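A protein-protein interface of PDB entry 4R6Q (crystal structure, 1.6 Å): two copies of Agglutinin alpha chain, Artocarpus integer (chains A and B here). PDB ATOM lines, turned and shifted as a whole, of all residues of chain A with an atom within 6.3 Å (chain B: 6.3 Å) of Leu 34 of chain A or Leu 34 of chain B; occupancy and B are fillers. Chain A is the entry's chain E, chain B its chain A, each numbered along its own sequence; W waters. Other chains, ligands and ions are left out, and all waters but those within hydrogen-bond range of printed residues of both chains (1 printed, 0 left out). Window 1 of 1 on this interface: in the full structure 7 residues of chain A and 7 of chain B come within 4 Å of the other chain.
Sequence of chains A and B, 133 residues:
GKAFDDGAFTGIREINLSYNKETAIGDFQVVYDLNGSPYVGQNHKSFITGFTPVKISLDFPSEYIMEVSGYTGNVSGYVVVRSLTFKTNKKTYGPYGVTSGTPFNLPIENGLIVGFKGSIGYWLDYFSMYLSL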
ATOM      1  N   ASP A   6     -14.071  -7.213  13.775  1.00  0.00           N
ATOM      2  CA  ASP A   6     -14.622  -8.376  14.393  1.00  0.00           C
ATOM      3  C   ASP A   6     -13.545  -9.064  15.297  1.00  0.00           C
ATOM      4  O   ASP A   6     -13.897  -9.802  16.214  1.00  0.00           O
ATOM      5  CB  ASP A   6     -15.051  -9.379  13.307  1.00  0.00           C
ATOM      6  CG  ASP A   6     -16.376  -9.010  12.598  1.00  0.00           C
ATOM      7  OD1 ASP A   6     -17.106  -8.087  13.070  1.00  0.00           O
ATOM      8  OD2 ASP A   6     -16.683  -9.683  11.563  1.00  0.00           O
ATOM      9  N   ALA A   8     -10.420 -11.895  15.702  1.00  0.00           N
ATOM     10  CA  ALA A   8      -9.992 -13.159  15.157  1.00  0.00           C
ATOM     11  C   ALA A   8     -10.717 -14.328  15.845  1.00  0.00           C
ATOM     12  O   ALA A   8     -10.966 -14.310  17.076  1.00  0.00           O
ATOM     13  CB  ALA A   8      -8.446 -13.264  15.263  1.00  0.00           C
ATOM     14  N   PHE A   9     -11.046 -15.342  15.024  1.00  0.00           N
ATOM     15  CA  PHE A   9     -11.757 -16.449  15.481  1.00  0.00           C
ATOM     16  C   PHE A   9     -11.008 -17.686  15.006  1.00  0.00           C
ATOM     17  O   PHE A   9      -9.826 -17.592  14.729  1.00  0.00           O
ATOM     18  CB  PHE A   9     -13.182 -16.324  14.908  1.00  0.00           C
ATOM     19  CG  PHE A   9     -13.939 -15.196  15.524  1.00  0.00           C
ATOM     20  CD1 PHE A   9     -13.890 -13.972  14.924  1.00  0.00           C
ATOM     21  CD2 PHE A   9     -14.749 -15.335  16.691  1.00  0.00           C
ATOM     22  CE1 PHE A   9     -14.562 -12.899  15.445  1.00  0.00           C
ATOM     23  CE2 PHE A   9     -15.423 -14.245  17.214  1.00  0.00           C
ATOM     24  CZ  PHE A   9     -15.293 -13.008  16.587  1.00  0.00           C
ATOM     25  N   THR A  10     -11.688 -18.818  14.974  1.00  0.00           N
ATOM     26  CA  THR A  10     -11.001 -19.988  14.618  1.00  0.00           C
ATOM     27  C   THR A  10     -11.352 -20.448  13.223  1.00  0.00           C
ATOM     28  O   THR A  10     -10.799 -21.418  12.776  1.00  0.00           O
ATOM     29  CB  THR A  10     -11.132 -21.062  15.679  1.00  0.00           C
ATOM     30  OG1 THR A  10     -12.467 -21.387  15.824  1.00  0.00           O
ATOM     31  CG2 THR A  10     -10.634 -20.519  17.035  1.00  0.00           C
ATOM     32  N   GLY A  11     -12.254 -19.727  12.548  1.00  0.00           N
ATOM     33  CA  GLY A  11     -12.447 -19.885  11.097  1.00  0.00           C
ATOM     34  C   GLY A  11     -13.810 -19.332  10.728  1.00  0.00           C
ATOM     35  O   GLY A  11     -14.383 -18.581  11.453  1.00  0.00           O
ATOM     36  N   ARG A  13     -17.702 -19.955   9.054  1.00  0.00           N
ATOM     37  CA  ARG A  13     -18.834 -20.795   8.637  1.00  0.00           C
ATOM     38  C   ARG A  13     -19.721 -20.183   7.546  1.00  0.00           C
ATOM     39  O   ARG A  13     -20.151 -20.910   6.643  1.00  0.00           O
ATOM     40  CB  ARG A  13     -19.657 -21.121   9.888  1.00  0.00           C
ATOM     41  CG  ARG A  13     -18.946 -22.171  10.746  1.00  0.00           C
ATOM     42  CD  ARG A  13     -19.543 -22.134  12.135  1.00  0.00           C
ATOM     43  NE  ARG A  13     -19.022 -23.207  12.994  1.00  0.00           N
ATOM     44  CZ  ARG A  13     -19.412 -24.480  13.009  1.00  0.00           C
ATOM     45  NH1 ARG A  13     -20.367 -24.905  12.182  1.00  0.00           N
ATOM     46  NH2 ARG A  13     -18.807 -25.334  13.848  1.00  0.00           N
ATOM     47  N   TYR A  32     -18.665 -16.794  12.211  1.00  0.00           N
ATOM     48  CA  TYR A  32     -17.375 -17.434  12.440  1.00  0.00           C
ATOM     49  C   TYR A  32     -17.481 -18.832  13.061  1.00  0.00           C
ATOM     50  O   TYR A  32     -18.546 -19.198  13.648  1.00  0.00           O
ATOM     51  CB  TYR A  32     -16.660 -16.525  13.404  1.00  0.00           C
ATOM     52  CG  TYR A  32     -16.264 -15.196  12.755  1.00  0.00           C
ATOM     53  CD1 TYR A  32     -15.263 -15.173  11.828  1.00  0.00           C
ATOM     54  CD2 TYR A  32     -16.969 -14.018  13.029  1.00  0.00           C
ATOM     55  CE1 TYR A  32     -14.852 -14.029  11.182  1.00  0.00           C
ATOM     56  CE2 TYR A  32     -16.605 -12.810  12.418  1.00  0.00           C
ATOM     57  CZ  TYR A  32     -15.554 -12.826  11.531  1.00  0.00           C
ATOM     58  OH  TYR A  32     -15.234 -11.657  10.959  1.00  0.00           O
ATOM     59  N   ASP A  33     -16.396 -19.627  12.988  1.00  0.00           N
ATOM     60  CA  ASP A  33     -16.304 -20.717  13.950  1.00  0.00           C
ATOM     61  C   ASP A  33     -15.517 -20.166  15.197  1.00  0.00           C
ATOM     62  O   ASP A  33     -14.489 -19.471  15.036  1.00  0.00           O
ATOM     63  CB  ASP A  33     -15.512 -21.833  13.385  1.00  0.00           C
ATOM     64  CG  ASP A  33     -15.512 -23.040  14.345  1.00  0.00           C
ATOM     65  OD1 ASP A  33     -16.639 -23.546  14.654  1.00  0.00           O
ATOM     66  OD2 ASP A  33     -14.427 -23.420  14.869  1.00  0.00           O
ATOM     67  N   LEU A  34     -15.932 -20.567  16.404  1.00  0.00           N
ATOM     68  CA  LEU A  34     -15.111 -20.342  17.561  1.00  0.00           C
ATOM     69  C   LEU A  34     -14.992 -21.675  18.306  1.00  0.00           C
ATOM     70  O   LEU A  34     -15.958 -22.107  18.950  1.00  0.00           O
ATOM     71  CB  LEU A  34     -15.763 -19.278  18.435  1.00  0.00           C
ATOM     72  CG  LEU A  34     -14.973 -18.856  19.704  1.00  0.00           C
ATOM     73  CD1 LEU A  34     -13.626 -18.268  19.418  1.00  0.00           C
ATOM     74  CD2 LEU A  34     -15.851 -17.925  20.494  1.00  0.00           C
ATOM     75  N   ASN A  35     -13.817 -22.273  18.230  1.00  0.00           N
ATOM     76  CA  ASN A  35     -13.530 -23.493  19.018  1.00  0.00           C
ATOM     77  C   ASN A  35     -14.553 -24.598  18.736  1.00  0.00           C
ATOM     78  O   ASN A  35     -14.925 -25.358  19.608  1.00  0.00           O
ATOM     79  CB  ASN A  35     -13.406 -23.113  20.512  1.00  0.00           C
ATOM     80  CG  ASN A  35     -12.298 -22.082  20.711  1.00  0.00           C
ATOM     81  OD1 ASN A  35     -11.178 -22.291  20.195  1.00  0.00           O
ATOM     82  ND2 ASN A  35     -12.574 -20.994  21.446  1.00  0.00           N
ATOM     83  N   GLY A  36     -14.998 -24.634  17.476  1.00  0.00           N
ATOM     84  CA  GLY A  36     -15.925 -25.661  17.016  1.00  0.00           C
ATOM     85  C   GLY A  36     -17.404 -25.327  17.141  1.00  0.00           C
ATOM     86  O   GLY A  36     -18.244 -26.137  16.773  1.00  0.00           O
ATOM     87  N   SER A  37     -17.746 -24.149  17.635  1.00  0.00           N
ATOM     88  CA  SER A  37     -19.127 -23.752  17.679  1.00  0.00           C
ATOM     89  C   SER A  37     -19.349 -22.500  16.868  1.00  0.00           C
ATOM     90  O   SER A  37     -18.428 -21.666  16.732  1.00  0.00           O
ATOM     91  CB  SER A  37     -19.563 -23.434  19.092  1.00  0.00           C
ATOM     92  OG  SER A  37     -19.187 -24.493  19.941  1.00  0.00           O
ATOM     93  N   PRO A  38     -20.571 -22.344  16.347  1.00  0.00           N
ATOM     94  CA  PRO A  38     -20.839 -21.076  15.631  1.00  0.00           C
ATOM     95  C   PRO A  38     -20.879 -19.817  16.484  1.00  0.00           C
ATOM     96  O   PRO A  38     -21.322 -19.823  17.623  1.00  0.00           O
ATOM     97  CB  PRO A  38     -22.176 -21.323  14.896  1.00  0.00           C
ATOM     98  CG  PRO A  38     -22.737 -22.575  15.452  1.00  0.00           C
ATOM     99  CD  PRO A  38     -21.666 -23.334  16.196  1.00  0.00           C
ATOM    100  N   TYR A  39     -20.282 -18.755  15.973  1.00  0.00           N
ATOM    101  CA  TYR A  39     -20.304 -17.474  16.624  1.00  0.00           C
ATOM    102  C   TYR A  39     -20.835 -16.462  15.566  1.00  0.00           C
ATOM    103  O   TYR A  39     -20.176 -16.202  14.531  1.00  0.00           O
ATOM    104  CB  TYR A  39     -18.878 -17.095  17.089  1.00  0.00           C
ATOM    105  CG  TYR A  39     -18.921 -15.782  17.806  1.00  0.00           C
ATOM    106  CD1 TYR A  39     -18.915 -14.571  17.095  1.00  0.00           C
ATOM    107  CD2 TYR A  39     -19.037 -15.738  19.207  1.00  0.00           C
ATOM    108  CE1 TYR A  39     -18.995 -13.359  17.725  1.00  0.00           C
ATOM    109  CE2 TYR A  39     -19.114 -14.510  19.861  1.00  0.00           C
ATOM    110  CZ  TYR A  39     -19.137 -13.345  19.121  1.00  0.00           C
ATOM    111  OH  TYR A  39     -19.200 -12.141  19.748  1.00  0.00           O
ATOM    112  N   ALA B   8      -9.311 -21.887  22.459  1.00  0.00           N
ATOM    113  CA  ALA B   8      -8.431 -20.724  22.492  1.00  0.00           C
ATOM    114  C   ALA B   8      -9.218 -19.415  22.307  1.00  0.00           C
ATOM    115  O   ALA B   8     -10.160 -19.336  21.491  1.00  0.00           O
ATOM    116  CB  ALA B   8      -7.407 -20.837  21.399  1.00  0.00           C
ATOM    117  N   PHE B   9      -8.726 -18.411  23.005  1.00  0.00           N
ATOM    118  CA  PHE B   9      -9.305 -17.058  23.050  1.00  0.00           C
ATOM    119  C   PHE B   9      -8.245 -16.016  22.866  1.00  0.00           C
ATOM    120  O   PHE B   9      -7.158 -16.284  22.366  1.00  0.00           O
ATOM    121  CB  PHE B   9     -10.042 -16.875  24.369  1.00  0.00           C
ATOM    122  CG  PHE B   9     -11.163 -17.822  24.515  1.00  0.00           C
ATOM    123  CD1 PHE B   9     -10.948 -19.124  25.083  1.00  0.00           C
ATOM    124  CD2 PHE B   9     -12.422 -17.481  24.039  1.00  0.00           C
ATOM    125  CE1 PHE B   9     -11.983 -20.032  25.128  1.00  0.00           C
ATOM    126  CE2 PHE B   9     -13.476 -18.417  24.105  1.00  0.00           C
ATOM    127  CZ  PHE B   9     -13.250 -19.692  24.651  1.00  0.00           C
ATOM    128  N   THR B  10      -8.562 -14.790  23.253  1.00  0.00           N
ATOM    129  CA  THR B  10      -7.604 -13.712  22.995  1.00  0.00           C
ATOM    130  C   THR B  10      -6.765 -13.401  24.232  1.00  0.00           C
ATOM    131  O   THR B  10      -5.828 -12.630  24.158  1.00  0.00           O
ATOM    132  CB  THR B  10      -8.343 -12.382  22.645  1.00  0.00           C
ATOM    133  OG1 THR B  10      -9.301 -12.587  21.619  1.00  0.00           O
ATOM    134  CG2 THR B  10      -7.355 -11.344  22.230  1.00  0.00           C
ATOM    135  N   GLY B  11      -7.080 -13.995  25.379  1.00  0.00           N
ATOM    136  CA  GLY B  11      -6.465 -13.566  26.629  1.00  0.00           C
ATOM    137  C   GLY B  11      -7.313 -14.042  27.771  1.00  0.00           C
ATOM    138  O   GLY B  11      -8.338 -14.697  27.554  1.00  0.00           O
ATOM    139  N   ARG B  13      -9.097 -12.797  31.481  1.00  0.00           N
ATOM    140  CA  ARG B  13      -9.581 -11.750  32.406  1.00  0.00           C
ATOM    141  C   ARG B  13      -9.678 -12.150  33.879  1.00  0.00           C
ATOM    142  O   ARG B  13      -9.388 -11.376  34.801  1.00  0.00           O
ATOM    143  CB  ARG B  13     -10.943 -11.203  31.935  1.00  0.00           C
ATOM    144  CG  ARG B  13     -10.781 -10.429  30.644  1.00  0.00           C
ATOM    145  CD  ARG B  13     -12.146 -10.161  30.028  1.00  0.00           C
ATOM    146  NE  ARG B  13     -12.053  -9.234  28.890  1.00  0.00           N
ATOM    147  CZ  ARG B  13     -12.066  -7.899  28.979  1.00  0.00           C
ATOM    148  NH1 ARG B  13     -12.026  -7.194  27.867  1.00  0.00           N
ATOM    149  NH2 ARG B  13     -12.124  -7.255  30.157  1.00  0.00           N
ATOM    150  N   TYR B  32     -12.449 -15.538  29.851  1.00  0.00           N
ATOM    151  CA  TYR B  32     -11.514 -15.170  28.773  1.00  0.00           C
ATOM    152  C   TYR B  32     -11.758 -13.747  28.258  1.00  0.00           C
ATOM    153  O   TYR B  32     -12.779 -13.081  28.552  1.00  0.00           O
ATOM    154  CB  TYR B  32     -11.580 -16.168  27.618  1.00  0.00           C
ATOM    155  CG  TYR B  32     -11.147 -17.581  28.043  1.00  0.00           C
ATOM    156  CD1 TYR B  32      -9.814 -17.909  28.210  1.00  0.00           C
ATOM    157  CD2 TYR B  32     -12.114 -18.530  28.384  1.00  0.00           C
ATOM    158  CE1 TYR B  32      -9.446 -19.196  28.635  1.00  0.00           C
ATOM    159  CE2 TYR B  32     -11.759 -19.826  28.784  1.00  0.00           C
ATOM    160  CZ  TYR B  32     -10.412 -20.141  28.873  1.00  0.00           C
ATOM    161  OH  TYR B  32     -10.041 -21.402  29.293  1.00  0.00           O
ATOM    162  N   ASP B  33     -10.773 -13.219  27.543  1.00  0.00           N
ATOM    163  CA  ASP B  33     -11.104 -12.182  26.612  1.00  0.00           C
ATOM    164  C   ASP B  33     -11.330 -12.776  25.253  1.00  0.00           C
ATOM    165  O   ASP B  33     -10.575 -13.702  24.827  1.00  0.00           O
ATOM    166  CB  ASP B  33      -9.972 -11.160  26.495  1.00  0.00           C
ATOM    167  CG  ASP B  33     -10.371  -9.991  25.631  1.00  0.00           C
ATOM    168  OD1 ASP B  33     -11.257  -9.208  26.052  1.00  0.00           O
ATOM    169  OD2 ASP B  33      -9.774  -9.866  24.519  1.00  0.00           O
ATOM    170  N   LEU B  34     -12.283 -12.197  24.507  1.00  0.00           N
ATOM    171  CA  LEU B  34     -12.473 -12.586  23.100  1.00  0.00           C
ATOM    172  C   LEU B  34     -12.616 -11.297  22.289  1.00  0.00           C
ATOM    173  O   LEU B  34     -13.672 -10.696  22.291  1.00  0.00           O
ATOM    174  CB  LEU B  34     -13.707 -13.486  22.925  1.00  0.00           C
ATOM    175  CG  LEU B  34     -13.987 -13.915  21.427  1.00  0.00           C
ATOM    176  CD1 LEU B  34     -12.902 -14.739  20.796  1.00  0.00           C
ATOM    177  CD2 LEU B  34     -15.422 -14.507  21.351  1.00  0.00           C
ATOM    178  N   ASN B  35     -11.539 -10.882  21.658  1.00  0.00           N
ATOM    179  CA  ASN B  35     -11.537  -9.655  20.856  1.00  0.00           C
ATOM    180  C   ASN B  35     -12.071  -8.442  21.585  1.00  0.00           C
ATOM    181  O   ASN B  35     -12.802  -7.631  21.013  1.00  0.00           O
ATOM    182  CB  ASN B  35     -12.181  -9.891  19.501  1.00  0.00           C
ATOM    183  CG  ASN B  35     -11.564 -11.108  18.814  1.00  0.00           C
ATOM    184  OD1 ASN B  35     -10.343 -11.143  18.686  1.00  0.00           O
ATOM    185  ND2 ASN B  35     -12.382 -12.092  18.455  1.00  0.00           N
ATOM    186  N   GLY B  36     -11.709  -8.301  22.845  1.00  0.00           N
ATOM    187  CA  GLY B  36     -12.141  -7.131  23.603  1.00  0.00           C
ATOM    188  C   GLY B  36     -13.386  -7.311  24.466  1.00  0.00           C
ATOM    189  O   GLY B  36     -13.635  -6.471  25.319  1.00  0.00           O
ATOM    190  N   SER B  37     -14.143  -8.386  24.278  1.00  0.00           N
ATOM    191  CA  SER B  37     -15.289  -8.706  25.145  1.00  0.00           C
ATOM    192  C   SER B  37     -14.989  -9.854  26.113  1.00  0.00           C
ATOM    193  O   SER B  37     -14.325 -10.824  25.730  1.00  0.00           O
ATOM    194  CB  SER B  37     -16.492  -9.178  24.337  1.00  0.00           C
ATOM    195  OG  SER B  37     -16.888  -8.110  23.481  1.00  0.00           O
ATOM    196  N   PRO B  38     -15.550  -9.778  27.324  1.00  0.00           N
ATOM    197  CA  PRO B  38     -15.444 -10.950  28.217  1.00  0.00           C
ATOM    198  C   PRO B  38     -16.136 -12.179  27.699  1.00  0.00           C
ATOM    199  O   PRO B  38     -17.198 -12.081  27.088  1.00  0.00           O
ATOM    200  CB  PRO B  38     -16.033 -10.465  29.531  1.00  0.00           C
ATOM    201  CG  PRO B  38     -15.968  -8.942  29.471  1.00  0.00           C
ATOM    202  CD  PRO B  38     -16.080  -8.584  28.007  1.00  0.00           C
ATOM    203  N   TYR B  39     -15.479 -13.320  27.727  1.00  0.00           N
ATOM    204  CA  TYR B  39     -16.129 -14.495  27.303  1.00  0.00           C
ATOM    205  C   TYR B  39     -16.255 -15.369  28.539  1.00  0.00           C
ATOM    206  O   TYR B  39     -15.249 -15.835  29.087  1.00  0.00           O
ATOM    207  CB  TYR B  39     -15.328 -15.218  26.218  1.00  0.00           C
ATOM    208  CG  TYR B  39     -15.991 -16.476  25.695  1.00  0.00           C
ATOM    209  CD1 TYR B  39     -16.055 -17.663  26.472  1.00  0.00           C
ATOM    210  CD2 TYR B  39     -16.603 -16.466  24.445  1.00  0.00           C
ATOM    211  CE1 TYR B  39     -16.654 -18.831  25.984  1.00  0.00           C
ATOM    212  CE2 TYR B  39     -17.200 -17.610  23.952  1.00  0.00           C
ATOM    213  CZ  TYR B  39     -17.247 -18.769  24.704  1.00  0.00           C
ATOM    214  OH  TYR B  39     -17.852 -19.859  24.100  1.00  0.00           O
HETATM  215  O   HOH W   1     -15.728 -21.513  22.540  1.00  0.00           O
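Among the printed residues, pairs that only touch across the chains: Asn 35 of chain A with Phe 9 of chain B (3.5 Å), Asp 6 of chain A with Asn 35 of chain B (3.5 Å), Leu 34 of chain A with Leu 34 of chain B (3.5 Å), Phe 9 of chain A with Asn 35 of chain B (3.6 Å), Leu 34 of chain A with Tyr 39 of chain B (3.7 Å) and Tyr 39 of chain A with Leu 34 of chain B (3.98 Å).
The backbone carbonyl oxygen (O) of Ala 8 of chain A sits at hydrogen-bond distance from the side-chain amide nitrogen (ND2) of Asn 35 of chain B, at 3.0 Å. The side-chain amide nitrogen (ND2) of Asn 35 of chain A sits at hydrogen-bond distance from the backbone carbonyl oxygen (O) of Ala 8 of chain B.
Water W1 lies within hydrogen-bond range of OH of Tyr 39 of chain B (3.1 Å) and ND2 of Asn 35 of chain A (3.4 Å).
The backbone NH of Asn 35 of chain B sits at hydrogen-bond distance from the side-chain hydroxyl of Thr 10 of chain B (2.8 Å). The backbone carbonyl oxygen of Tyr 39 of chain A lies within hydrogen-bond range of the backbone NH of Tyr 32 of chain A (2.8 Å). OG1 of Thr 10 of chain A is in hydrogen-bond range of N of Asn 35 of chain A (2.9 Å). The backbone carbonyl oxygen of Tyr 32 of chain B lies within hydrogen-bond range of the backbone NH of Tyr 39 of chain B (2.8 Å). The side-chain carboxylate (OD2) of Asp 6 of chain A lies within hydrogen-bond range of the side-chain hydroxyl (OH) of Tyr 32 of chain A (2.5 Å).
Ala 8 of chain A touches Asn 35 of chain B, and with the chains exchanged Asn 35 of chain A touches Ala 8 of chain B. Phe 9 of chain A touches Asn 35 of chain B, and with the chains exchanged Asn 35 of chain A touches Phe 9 of chain B. Leu 34 of chain A touches its own counterpart, Leu 34 of chain B. Leu 34 of chain A touches Tyr 39 of chain B, and with the chains exchanged Tyr 39 of chain A touches Leu 34 of chain B. Positions printed for both chains: 8, 9, 10, 11, 13, 32, 33, 34, 35, 36, 37, 38 and 39.
Leu 34 of chain A touches just these residues of chain B: Leu 34 and Tyr 39. Of the printed residues of chain B, Tyr 39 of chain A touches Leu 34. Printed residues of chain B within 4 Å of Asn 35 of chain A: Ala 8 (2.9 Å) and Phe 9 (3.5 Å). Printed residues of chain A within 4 Å of Tyr 39 of chain B: Leu 34.
Of the 14 printed residues of chain A, 6 touch a printed residue of chain B. Hydrophobic or aromatic side chains of chain A that line the printed part of chain B: Phe 9, Leu 34 and Tyr 39. Printed residues of chain B that touch a printed residue of chain A: Ala 8, Phe 9, Leu 34, Asn 35 and Tyr 39. Among the printed residues, no Asp or Glu carboxylate lies within 4 Å of a Lys or Arg side-chain nitrogen of the other chain.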
